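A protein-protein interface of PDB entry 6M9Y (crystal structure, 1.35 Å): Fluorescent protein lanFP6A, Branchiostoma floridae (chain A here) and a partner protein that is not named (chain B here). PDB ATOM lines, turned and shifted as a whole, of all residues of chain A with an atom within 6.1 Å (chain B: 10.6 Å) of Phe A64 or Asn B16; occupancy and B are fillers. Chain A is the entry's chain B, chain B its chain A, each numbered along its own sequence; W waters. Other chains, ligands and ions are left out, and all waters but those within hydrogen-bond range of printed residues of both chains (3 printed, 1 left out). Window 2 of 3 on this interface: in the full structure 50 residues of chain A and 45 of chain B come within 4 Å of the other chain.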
ATOM      1  N   TYR A  34      -7.555  33.502   5.987  1.00  0.00           N
ATOM      2  CA  TYR A  34      -6.900  34.216   7.117  1.00  0.00           C
ATOM      3  C   TYR A  34      -7.041  35.731   6.975  1.00  0.00           C
ATOM      4  O   TYR A  34      -7.186  36.233   5.899  1.00  0.00           O
ATOM      5  CB  TYR A  34      -5.442  33.768   7.277  1.00  0.00           C
ATOM      6  CG  TYR A  34      -5.382  32.360   7.795  1.00  0.00           C
ATOM      7  CD1 TYR A  34      -5.481  32.097   9.142  1.00  0.00           C
ATOM      8  CD2 TYR A  34      -5.314  31.291   6.923  1.00  0.00           C
ATOM      9  CE1 TYR A  34      -5.521  30.801   9.617  1.00  0.00           C
ATOM     10  CE2 TYR A  34      -5.312  29.992   7.388  1.00  0.00           C
ATOM     11  CZ  TYR A  34      -5.446  29.752   8.729  1.00  0.00           C
ATOM     12  OH  TYR A  34      -5.493  28.487   9.211  1.00  0.00           O
ATOM     13  N   ASP A  36      -5.002  38.159   7.139  1.00  0.00           N
ATOM     14  CA  ASP A  36      -3.933  38.876   6.432  1.00  0.00           C
ATOM     15  C   ASP A  36      -3.862  38.471   4.960  1.00  0.00           C
ATOM     16  O   ASP A  36      -2.847  38.729   4.288  1.00  0.00           O
ATOM     17  CB  ASP A  36      -2.587  38.758   7.157  1.00  0.00           C
ATOM     18  CG  ASP A  36      -2.159  37.364   7.525  1.00  0.00           C
ATOM     19  OD1 ASP A  36      -2.835  36.395   7.186  1.00  0.00           O
ATOM     20  OD2 ASP A  36      -1.093  37.320   8.221  1.00  0.00           O
ATOM     21  N   ALA A  38      -3.812  35.559   3.447  1.00  0.00           N
ATOM     22  CA  ALA A  38      -3.387  34.185   3.218  1.00  0.00           C
ATOM     23  C   ALA A  38      -4.579  33.248   3.235  1.00  0.00           C
ATOM     24  O   ALA A  38      -5.584  33.546   3.899  1.00  0.00           O
ATOM     25  CB  ALA A  38      -2.412  33.792   4.305  1.00  0.00           C
ATOM     26  N   PHE A  39      -4.446  32.120   2.539  1.00  0.00           N
ATOM     27  CA  PHE A  39      -5.482  31.100   2.633  1.00  0.00           C
ATOM     28  C   PHE A  39      -4.820  29.717   2.611  1.00  0.00           C
ATOM     29  O   PHE A  39      -3.756  29.502   2.034  1.00  0.00           O
ATOM     30  CB  PHE A  39      -6.581  31.252   1.574  1.00  0.00           C
ATOM     31  CG  PHE A  39      -6.129  31.271   0.146  1.00  0.00           C
ATOM     32  CD1 PHE A  39      -5.827  32.483  -0.480  1.00  0.00           C
ATOM     33  CD2 PHE A  39      -6.079  30.095  -0.612  1.00  0.00           C
ATOM     34  CE1 PHE A  39      -5.457  32.514  -1.817  1.00  0.00           C
ATOM     35  CE2 PHE A  39      -5.735  30.153  -1.960  1.00  0.00           C
ATOM     36  CZ  PHE A  39      -5.417  31.356  -2.548  1.00  0.00           C
ATOM     37  N   VAL A  40      -5.543  28.796   3.221  1.00  0.00           N
ATOM     38  CA  VAL A  40      -5.192  27.386   3.251  1.00  0.00           C
ATOM     39  C   VAL A  40      -6.352  26.592   2.640  1.00  0.00           C
ATOM     40  O   VAL A  40      -7.525  26.813   2.978  1.00  0.00           O
ATOM     41  CB  VAL A  40      -4.876  26.898   4.678  1.00  0.00           C
ATOM     42  CG1 VAL A  40      -4.847  25.386   4.774  1.00  0.00           C
ATOM     43  CG2 VAL A  40      -3.585  27.465   5.223  1.00  0.00           C
ATOM     44  N   GLY A  61      -0.963  26.014   1.874  1.00  0.00           N
ATOM     45  CA  GLY A  61      -1.173  27.391   2.287  1.00  0.00           C
ATOM     46  C   GLY A  61      -0.304  28.349   1.486  1.00  0.00           C
ATOM     47  O   GLY A  61       0.860  28.053   1.135  1.00  0.00           O
ATOM     48  N   THR A  62      -0.855  29.536   1.144  1.00  0.00           N
ATOM     49  CA  THR A  62      -0.143  30.547   0.434  1.00  0.00           C
ATOM     50  C   THR A  62      -0.509  31.945   0.938  1.00  0.00           C
ATOM     51  O   THR A  62      -1.548  32.157   1.580  1.00  0.00           O
ATOM     52  CB  THR A  62      -0.384  30.485  -1.105  1.00  0.00           C
ATOM     53  OG1 THR A  62      -1.811  30.593  -1.335  1.00  0.00           O
ATOM     54  CG2 THR A  62       0.143  29.204  -1.711  1.00  0.00           C
ATOM     55  N   GLY A  63       0.393  32.868   0.660  1.00  0.00           N
ATOM     56  CA  GLY A  63       0.170  34.291   0.948  1.00  0.00           C
ATOM     57  C   GLY A  63       0.415  34.681   2.373  1.00  0.00           C
ATOM     58  O   GLY A  63      -0.001  35.795   2.734  1.00  0.00           O
ATOM     59  N   PHE A  64       1.064  33.824   3.173  1.00  0.00           N
ATOM     60  CA  PHE A  64       1.365  34.212   4.540  1.00  0.00           C
ATOM     61  C   PHE A  64       2.502  35.222   4.545  1.00  0.00           C
ATOM     62  O   PHE A  64       3.559  35.002   3.956  1.00  0.00           O
ATOM     63  CB  PHE A  64       1.755  32.990   5.366  1.00  0.00           C
ATOM     64  CG  PHE A  64       0.579  32.110   5.661  1.00  0.00           C
ATOM     65  CD1 PHE A  64      -0.330  32.445   6.659  1.00  0.00           C
ATOM     66  CD2 PHE A  64       0.299  31.017   4.865  1.00  0.00           C
ATOM     67  CE1 PHE A  64      -1.434  31.657   6.926  1.00  0.00           C
ATOM     68  CE2 PHE A  64      -0.822  30.239   5.122  1.00  0.00           C
ATOM     69  CZ  PHE A  64      -1.669  30.540   6.153  1.00  0.00           C
ATOM     70  N   PRO A  65       2.305  36.426   5.145  1.00  0.00           N
ATOM     71  CA  PRO A  65       3.376  37.408   5.174  1.00  0.00           C
ATOM     72  C   PRO A  65       4.586  36.789   5.881  1.00  0.00           C
ATOM     73  O   PRO A  65       4.482  36.194   6.949  1.00  0.00           O
ATOM     74  CB  PRO A  65       2.792  38.575   5.965  1.00  0.00           C
ATOM     75  CG  PRO A  65       1.295  38.411   5.759  1.00  0.00           C
ATOM     76  CD  PRO A  65       1.087  36.914   5.792  1.00  0.00           C
ATOM     77  N   PRO A  66       5.811  37.042   5.332  1.00  0.00           N
ATOM     78  CA  PRO A  66       7.035  36.565   5.972  1.00  0.00           C
ATOM     79  C   PRO A  66       7.230  37.092   7.397  1.00  0.00           C
ATOM     80  O   PRO A  66       7.831  36.406   8.197  1.00  0.00           O
ATOM     81  CB  PRO A  66       8.141  37.045   5.030  1.00  0.00           C
ATOM     82  CG  PRO A  66       7.467  37.111   3.696  1.00  0.00           C
ATOM     83  CD  PRO A  66       6.049  37.545   3.977  1.00  0.00           C
ATOM     84  N   ASP A  67       6.664  38.257   7.711  1.00  0.00           N
ATOM     85  CA  ASP A  67       6.772  38.871   9.024  1.00  0.00           C
ATOM     86  C   ASP A  67       5.513  38.655   9.874  1.00  0.00           C
ATOM     87  O   ASP A  67       5.400  39.172  10.980  1.00  0.00           O
ATOM     88  CB  ASP A  67       7.055  40.366   8.862  1.00  0.00           C
ATOM     89  CG  ASP A  67       5.968  41.213   8.195  1.00  0.00           C
ATOM     90  OD1 ASP A  67       5.088  40.666   7.548  1.00  0.00           O
ATOM     91  OD2 ASP A  67       6.050  42.456   8.310  1.00  0.00           O
ATOM     92  N   GLY A  68       4.585  37.813   9.411  1.00  0.00           N
ATOM     93  CA  GLY A  68       3.370  37.575  10.163  1.00  0.00           C
ATOM     94  C   GLY A  68       3.524  36.434  11.176  1.00  0.00           C
ATOM     95  O   GLY A  68       4.578  35.792  11.281  1.00  0.00           O
ATOM     96  N   VAL A  70       2.348  33.412  11.515  1.00  0.00           N
ATOM     97  CA  VAL A  70       2.520  32.051  11.048  1.00  0.00           C
ATOM     98  C   VAL A  70       3.966  31.789  10.688  1.00  0.00           C
ATOM     99  O   VAL A  70       4.594  30.829  11.217  1.00  0.00           O
ATOM    100  CB  VAL A  70       1.562  31.729   9.894  1.00  0.00           C
ATOM    101  CG1 VAL A  70       1.898  30.351   9.303  1.00  0.00           C
ATOM    102  CG2 VAL A  70       0.138  31.775  10.427  1.00  0.00           C
ATOM    103  N   MET A  71       4.531  32.643   9.845  1.00  0.00           N
ATOM    104  CA  MET A  71       5.896  32.377   9.373  1.00  0.00           C
ATOM    105  C   MET A  71       6.944  32.702  10.442  1.00  0.00           C
ATOM    106  O   MET A  71       8.080  32.227  10.311  1.00  0.00           O
ATOM    107  CB  MET A  71       6.209  33.090   8.066  1.00  0.00           C
ATOM    108  CG  MET A  71       5.235  32.700   6.931  1.00  0.00           C
ATOM    109  SD  MET A  71       5.063  30.912   6.604  1.00  0.00           S
ATOM    110  CE  MET A  71       6.712  30.560   6.028  1.00  0.00           C
ATOM    111  N   TYR A 109      -5.342  36.017  15.990  1.00  0.00           N
ATOM    112  CA  TYR A 109      -5.163  35.805  14.587  1.00  0.00           C
ATOM    113  C   TYR A 109      -6.351  35.007  14.081  1.00  0.00           C
ATOM    114  O   TYR A 109      -6.517  33.892  14.520  1.00  0.00           O
ATOM    115  CB  TYR A 109      -3.814  35.133  14.320  1.00  0.00           C
ATOM    116  CG  TYR A 109      -3.466  34.930  12.868  1.00  0.00           C
ATOM    117  CD1 TYR A 109      -3.243  36.006  12.017  1.00  0.00           C
ATOM    118  CD2 TYR A 109      -3.337  33.662  12.313  1.00  0.00           C
ATOM    119  CE1 TYR A 109      -2.902  35.821  10.684  1.00  0.00           C
ATOM    120  CE2 TYR A 109      -2.939  33.450  11.006  1.00  0.00           C
ATOM    121  CZ  TYR A 109      -2.773  34.526  10.160  1.00  0.00           C
ATOM    122  OH  TYR A 109      -2.384  34.316   8.848  1.00  0.00           O
ATOM    123  N   GLY B  13       2.080  18.776   2.060  1.00  0.00           N
ATOM    124  CA  GLY B  13       1.655  19.864   1.202  1.00  0.00           C
ATOM    125  C   GLY B  13       2.760  20.889   1.171  1.00  0.00           C
ATOM    126  O   GLY B  13       3.925  20.528   1.045  1.00  0.00           O
ATOM    127  N   SER B  14       2.396  22.170   1.223  1.00  0.00           N
ATOM    128  CA  SER B  14       3.360  23.251   1.134  1.00  0.00           C
ATOM    129  C   SER B  14       2.763  24.482   1.781  1.00  0.00           C
ATOM    130  O   SER B  14       1.540  24.653   1.840  1.00  0.00           O
ATOM    131  CB  SER B  14       3.755  23.547  -0.296  1.00  0.00           C
ATOM    132  OG  SER B  14       2.636  23.990  -1.065  1.00  0.00           O
ATOM    133  N   PHE B  15       3.659  25.319   2.289  1.00  0.00           N
ATOM    134  CA  PHE B  15       3.312  26.670   2.821  1.00  0.00           C
ATOM    135  C   PHE B  15       4.196  27.690   2.105  1.00  0.00           C
ATOM    136  O   PHE B  15       5.395  27.557   2.107  1.00  0.00           O
ATOM    137  CB  PHE B  15       3.431  26.737   4.344  1.00  0.00           C
ATOM    138  CG  PHE B  15       2.175  26.271   5.028  1.00  0.00           C
ATOM    139  CD1 PHE B  15       1.916  24.930   5.186  1.00  0.00           C
ATOM    140  CD2 PHE B  15       1.237  27.174   5.485  1.00  0.00           C
ATOM    141  CE1 PHE B  15       0.730  24.502   5.742  1.00  0.00           C
ATOM    142  CE2 PHE B  15       0.045  26.746   6.036  1.00  0.00           C
ATOM    143  CZ  PHE B  15      -0.201  25.416   6.172  1.00  0.00           C
ATOM    144  N   ASN B  16       3.586  28.673   1.472  1.00  0.00           N
ATOM    145  CA  ASN B  16       4.325  29.682   0.764  1.00  0.00           C
ATOM    146  C   ASN B  16       5.275  29.021  -0.241  1.00  0.00           C
ATOM    147  O   ASN B  16       6.394  29.466  -0.439  1.00  0.00           O
ATOM    148  CB  ASN B  16       5.047  30.676   1.664  1.00  0.00           C
ATOM    149  CG  ASN B  16       4.130  31.645   2.365  1.00  0.00           C
ATOM    150  OD1 ASN B  16       2.887  31.568   2.243  1.00  0.00           O
ATOM    151  ND2 ASN B  16       4.750  32.614   3.018  1.00  0.00           N
ATOM    152  N   GLY B  17       4.806  27.965  -0.924  1.00  0.00           N
ATOM    153  CA  GLY B  17       5.580  27.339  -1.987  1.00  0.00           C
ATOM    154  C   GLY B  17       6.610  26.326  -1.547  1.00  0.00           C
ATOM    155  O   GLY B  17       7.210  25.729  -2.441  1.00  0.00           O
ATOM    156  N   VAL B  18       6.789  26.105  -0.249  1.00  0.00           N
ATOM    157  CA  VAL B  18       7.832  25.250   0.286  1.00  0.00           C
ATOM    158  C   VAL B  18       7.173  24.011   0.882  1.00  0.00           C
ATOM    159  O   VAL B  18       6.310  24.100   1.788  1.00  0.00           O
ATOM    160  CB  VAL B  18       8.708  26.003   1.298  1.00  0.00           C
ATOM    161  CG1 VAL B  18       9.759  25.105   1.924  1.00  0.00           C
ATOM    162  CG2 VAL B  18       9.372  27.190   0.651  1.00  0.00           C
ATOM    163  N   LYS B  19       7.593  22.833   0.394  1.00  0.00           N
ATOM    164  CA  LYS B  19       6.986  21.570   0.799  1.00  0.00           C
ATOM    165  C   LYS B  19       7.243  21.266   2.286  1.00  0.00           C
ATOM    166  O   LYS B  19       8.268  21.684   2.885  1.00  0.00           O
ATOM    167  CB  LYS B  19       7.525  20.407  -0.054  1.00  0.00           C
ATOM    168  CG  LYS B  19       7.160  20.523  -1.530  1.00  0.00           C
ATOM    169  CD  LYS B  19       7.562  19.351  -2.406  1.00  0.00           C
ATOM    170  CE  LYS B  19       7.073  19.540  -3.835  1.00  0.00           C
ATOM    171  NZ  LYS B  19       7.507  18.444  -4.741  1.00  0.00           N
ATOM    172  N   PHE B  20       6.306  20.516   2.879  1.00  0.00           N
ATOM    173  CA  PHE B  20       6.472  19.867   4.169  1.00  0.00           C
ATOM    174  C   PHE B  20       5.840  18.484   4.122  1.00  0.00           C
ATOM    175  O   PHE B  20       5.005  18.206   3.260  1.00  0.00           O
ATOM    176  CB  PHE B  20       5.868  20.692   5.321  1.00  0.00           C
ATOM    177  CG  PHE B  20       4.380  20.590   5.458  1.00  0.00           C
ATOM    178  CD1 PHE B  20       3.532  21.296   4.621  1.00  0.00           C
ATOM    179  CD2 PHE B  20       3.806  19.717   6.343  1.00  0.00           C
ATOM    180  CE1 PHE B  20       2.154  21.144   4.685  1.00  0.00           C
ATOM    181  CE2 PHE B  20       2.422  19.577   6.433  1.00  0.00           C
ATOM    182  CZ  PHE B  20       1.596  20.300   5.604  1.00  0.00           C
ATOM    183  N   LYS B  47       9.089  25.159   8.675  1.00  0.00           N
ATOM    184  CA  LYS B  47       9.450  26.554   8.505  1.00  0.00           C
ATOM    185  C   LYS B  47       8.345  27.527   8.894  1.00  0.00           C
ATOM    186  O   LYS B  47       8.520  28.705   8.740  1.00  0.00           O
ATOM    187  CB  LYS B  47       9.776  26.859   7.042  1.00  0.00           C
ATOM    188  CG  LYS B  47      11.008  26.126   6.533  1.00  0.00           C
ATOM    189  CD  LYS B  47      12.239  26.491   7.306  1.00  0.00           C
ATOM    190  CE  LYS B  47      13.473  26.543   6.428  1.00  0.00           C
ATOM    191  NZ  LYS B  47      14.480  27.504   6.942  1.00  0.00           N
ATOM    192  N   PHE B  48       7.241  27.032   9.419  1.00  0.00           N
ATOM    193  CA  PHE B  48       6.076  27.785   9.787  1.00  0.00           C
ATOM    194  C   PHE B  48       5.545  27.266  11.132  1.00  0.00           C
ATOM    195  O   PHE B  48       5.950  26.182  11.607  1.00  0.00           O
ATOM    196  CB  PHE B  48       4.979  27.653   8.716  1.00  0.00           C
ATOM    197  CG  PHE B  48       4.627  26.225   8.375  1.00  0.00           C
ATOM    198  CD1 PHE B  48       3.701  25.530   9.126  1.00  0.00           C
ATOM    199  CD2 PHE B  48       5.264  25.572   7.322  1.00  0.00           C
ATOM    200  CE1 PHE B  48       3.380  24.217   8.816  1.00  0.00           C
ATOM    201  CE2 PHE B  48       4.965  24.253   7.028  1.00  0.00           C
ATOM    202  CZ  PHE B  48       4.037  23.584   7.781  1.00  0.00           C
ATOM    203  N   SER B  49       4.649  28.033  11.752  1.00  0.00           N
ATOM    204  CA  SER B  49       4.085  27.674  13.037  1.00  0.00           C
ATOM    205  C   SER B  49       3.383  26.324  12.972  1.00  0.00           C
ATOM    206  O   SER B  49       2.428  26.185  12.250  1.00  0.00           O
ATOM    207  CB  SER B  49       3.131  28.701  13.551  1.00  0.00           C
ATOM    208  OG  SER B  49       2.472  28.235  14.693  1.00  0.00           O
ATOM    209  N   TYR B  51       1.177  25.379  14.912  1.00  0.00           N
ATOM    210  CA  TYR B  51      -0.223  25.667  15.245  1.00  0.00           C
ATOM    211  C   TYR B  51      -1.092  25.822  13.989  1.00  0.00           C
ATOM    212  O   TYR B  51      -2.285  25.570  14.077  1.00  0.00           O
ATOM    213  CB  TYR B  51      -0.345  26.928  16.120  1.00  0.00           C
ATOM    214  CG  TYR B  51      -0.059  26.628  17.576  1.00  0.00           C
ATOM    215  CD1 TYR B  51      -0.998  26.035  18.405  1.00  0.00           C
ATOM    216  CD2 TYR B  51       1.198  26.838  18.103  1.00  0.00           C
ATOM    217  CE1 TYR B  51      -0.693  25.686  19.723  1.00  0.00           C
ATOM    218  CE2 TYR B  51       1.517  26.522  19.416  1.00  0.00           C
ATOM    219  CZ  TYR B  51       0.570  25.943  20.259  1.00  0.00           C
ATOM    220  OH  TYR B  51       0.867  25.612  21.542  1.00  0.00           O
ATOM    221  N   ILE B  52      -0.508  26.185  12.842  1.00  0.00           N
ATOM    222  CA  ILE B  52      -1.309  26.346  11.607  1.00  0.00           C
ATOM    223  C   ILE B  52      -1.866  24.979  11.153  1.00  0.00           C
ATOM    224  O   ILE B  52      -2.837  24.923  10.425  1.00  0.00           O
ATOM    225  CB  ILE B  52      -0.511  27.073  10.494  1.00  0.00           C
ATOM    226  CG1 ILE B  52      -1.427  27.846   9.544  1.00  0.00           C
ATOM    227  CG2 ILE B  52       0.405  26.119   9.737  1.00  0.00           C
ATOM    228  CD1 ILE B  52      -2.283  28.904  10.258  1.00  0.00           C
ATOM    229  N   LEU B  53      -1.217  23.884  11.587  1.00  0.00           N
ATOM    230  CA  LEU B  53      -1.677  22.515  11.248  1.00  0.00           C
ATOM    231  C   LEU B  53      -2.749  21.987  12.187  1.00  0.00           C
ATOM    232  O   LEU B  53      -3.441  21.051  11.810  1.00  0.00           O
ATOM    233  CB  LEU B  53      -0.520  21.530  11.228  1.00  0.00           C
ATOM    234  CG  LEU B  53       0.607  21.826  10.245  1.00  0.00           C
ATOM    235  CD1 LEU B  53       1.692  20.767  10.350  1.00  0.00           C
ATOM    236  CD2 LEU B  53       0.054  21.898   8.829  1.00  0.00           C
ATOM    237  N   PRO B  55      -5.830  22.519  13.237  1.00  0.00           N
ATOM    238  CA  PRO B  55      -7.179  22.157  12.819  1.00  0.00           C
ATOM    239  C   PRO B  55      -7.294  20.995  11.846  1.00  0.00           C
ATOM    240  O   PRO B  55      -8.386  20.511  11.657  1.00  0.00           O
ATOM    241  CB  PRO B  55      -7.761  23.401  12.141  1.00  0.00           C
ATOM    242  CG  PRO B  55      -6.634  24.404  12.078  1.00  0.00           C
ATOM    243  CD  PRO B  55      -5.403  23.839  12.752  1.00  0.00           C
ATOM    244  N   HIS B  56      -6.154  20.589  11.255  1.00  0.00           N
ATOM    245  CA  HIS B  56      -6.062  19.498  10.337  1.00  0.00           C
ATOM    246  C   HIS B  56      -5.469  18.256  11.014  1.00  0.00           C
ATOM    247  O   HIS B  56      -5.105  17.314  10.320  1.00  0.00           O
ATOM    248  CB  HIS B  56      -5.186  19.909   9.147  1.00  0.00           C
ATOM    249  CG  HIS B  56      -5.642  21.208   8.576  1.00  0.00           C
ATOM    250  ND1 HIS B  56      -4.958  22.400   8.684  1.00  0.00           N
ATOM    251  CD2 HIS B  56      -6.775  21.483   7.891  1.00  0.00           C
ATOM    252  CE1 HIS B  56      -5.666  23.343   8.055  1.00  0.00           C
ATOM    253  NE2 HIS B  56      -6.768  22.816   7.581  1.00  0.00           N
HETATM  254  O   HOH W   1       2.183  26.688  -1.007  1.00  0.00           O
HETATM  255  O   HOH W   2      -4.575  25.922   8.491  1.00  0.00           O
HETATM  256  O   HOH W   3       2.654  31.968  -1.057  1.00  0.00           O
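Phe A64 touches just these residues of chain B: Phe B15 (3.7 Å) and Asn B16 (2.8 Å).
Asn B16 touches just these residues of chain A: Gly A61, Thr A62, Gly A63, Phe A64 and Met A71.
No residue of chain B comes within 4 Å of Ala A38.
Of chain B, only Asn B16 comes within 4 Å of Thr A62.
Gly A63 touches just one residue of chain B: Asn B16.
No residue of chain B comes within 4 Å of Pro A65.
Of the printed residues of chain B, Val A70 touches Phe B48 (3.7 Å), Ser B49 (2.8 Å) and Ile B52 (3.8 Å).
Of the printed residues of chain A, His B56 touches Val A40 (3.95 Å).
Printed residues of chain A within 4 Å of Ser B49: Val A70.
Of the printed residues of chain B, Met A71 touches Asn B16, Lys B47 and Phe B48.
OG of Ser B49 lies close to N of Tyr B51, at 3.1 Å.
O of Phe A39 lies within hydrogen-bond range of N of Thr A62, 3.0 Å away.
Among the printed residues, pairs that only touch across the chains: Tyr A34 with Ile B52, Val A40 with Phe B15, Val A40 with His B56, Gly A61 with Phe B15, Thr A62 with Asn B16, Phe A64 with Phe B15, Val A70 with Phe B48, Val A70 with Ile B52, Met A71 with Asn B16, Met A71 with Lys B47 and Met A71 with Phe B48.
Water W1 lies within hydrogen-bond range of the side-chain hydroxyl of Ser B14 (2.7 Å), the backbone carbonyl oxygen of Gly A61 (2.9 Å), the backbone NH of Gly B17 (2.9 Å) and the backbone NH of Asn B16 (3.5 Å).
Water W2 bridges O of Ile B52 (2.8 Å) and OH of Tyr A34 (2.8 Å).
Water W3 bridges the backbone NH (N) of Gly A63 (3.0 Å) and the side-chain amide oxygen (OD1) of Asn B16 (3.3 Å).
N of Gly A61 is in hydrogen-bond range of O of Ser B14 (2.8 Å).
The backbone NH (N) of Asn B16 sits at hydrogen-bond distance from the backbone carbonyl oxygen (O) of Gly A61, at 2.8 Å.
N of Gly A63 is in hydrogen-bond range of OD1 of Asn B16 (3.2 Å).
The side-chain amide nitrogen of Asn B16 is in hydrogen-bond range of the backbone carbonyl oxygen of Phe A64, 2.8 Å away.
N of Ser B49 sits at hydrogen-bond distance from O of Val A70, at 2.8 Å.
Of the 16 printed residues of chain A, 8 touch a printed residue of chain B.
Printed residues of chain A that touch a printed residue of chain B: Tyr A34, Val A40, Gly A61, Thr A62, Gly A63, Phe A64, Val A70 and Met A71.
Hydrophobic or aromatic side chains of chain A that line the printed part of chain B: Tyr A34, Val A40, Phe A64, Val A70 and Met A71.
Hydrophobic or aromatic side chains of chain B within 4 Å of the printed part of chain A: Phe B15, Phe B48, Ile B52 and His B56.
Along chain B the printed residues that touch a printed residue of chain A span positions 14 to 56.
Among the printed residues, 16 pairs touch across the chains.
Among the printed residues, no Asp or Glu carboxylate lies within 4 Å of a Lys or Arg side-chain nitrogen of the other chain.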
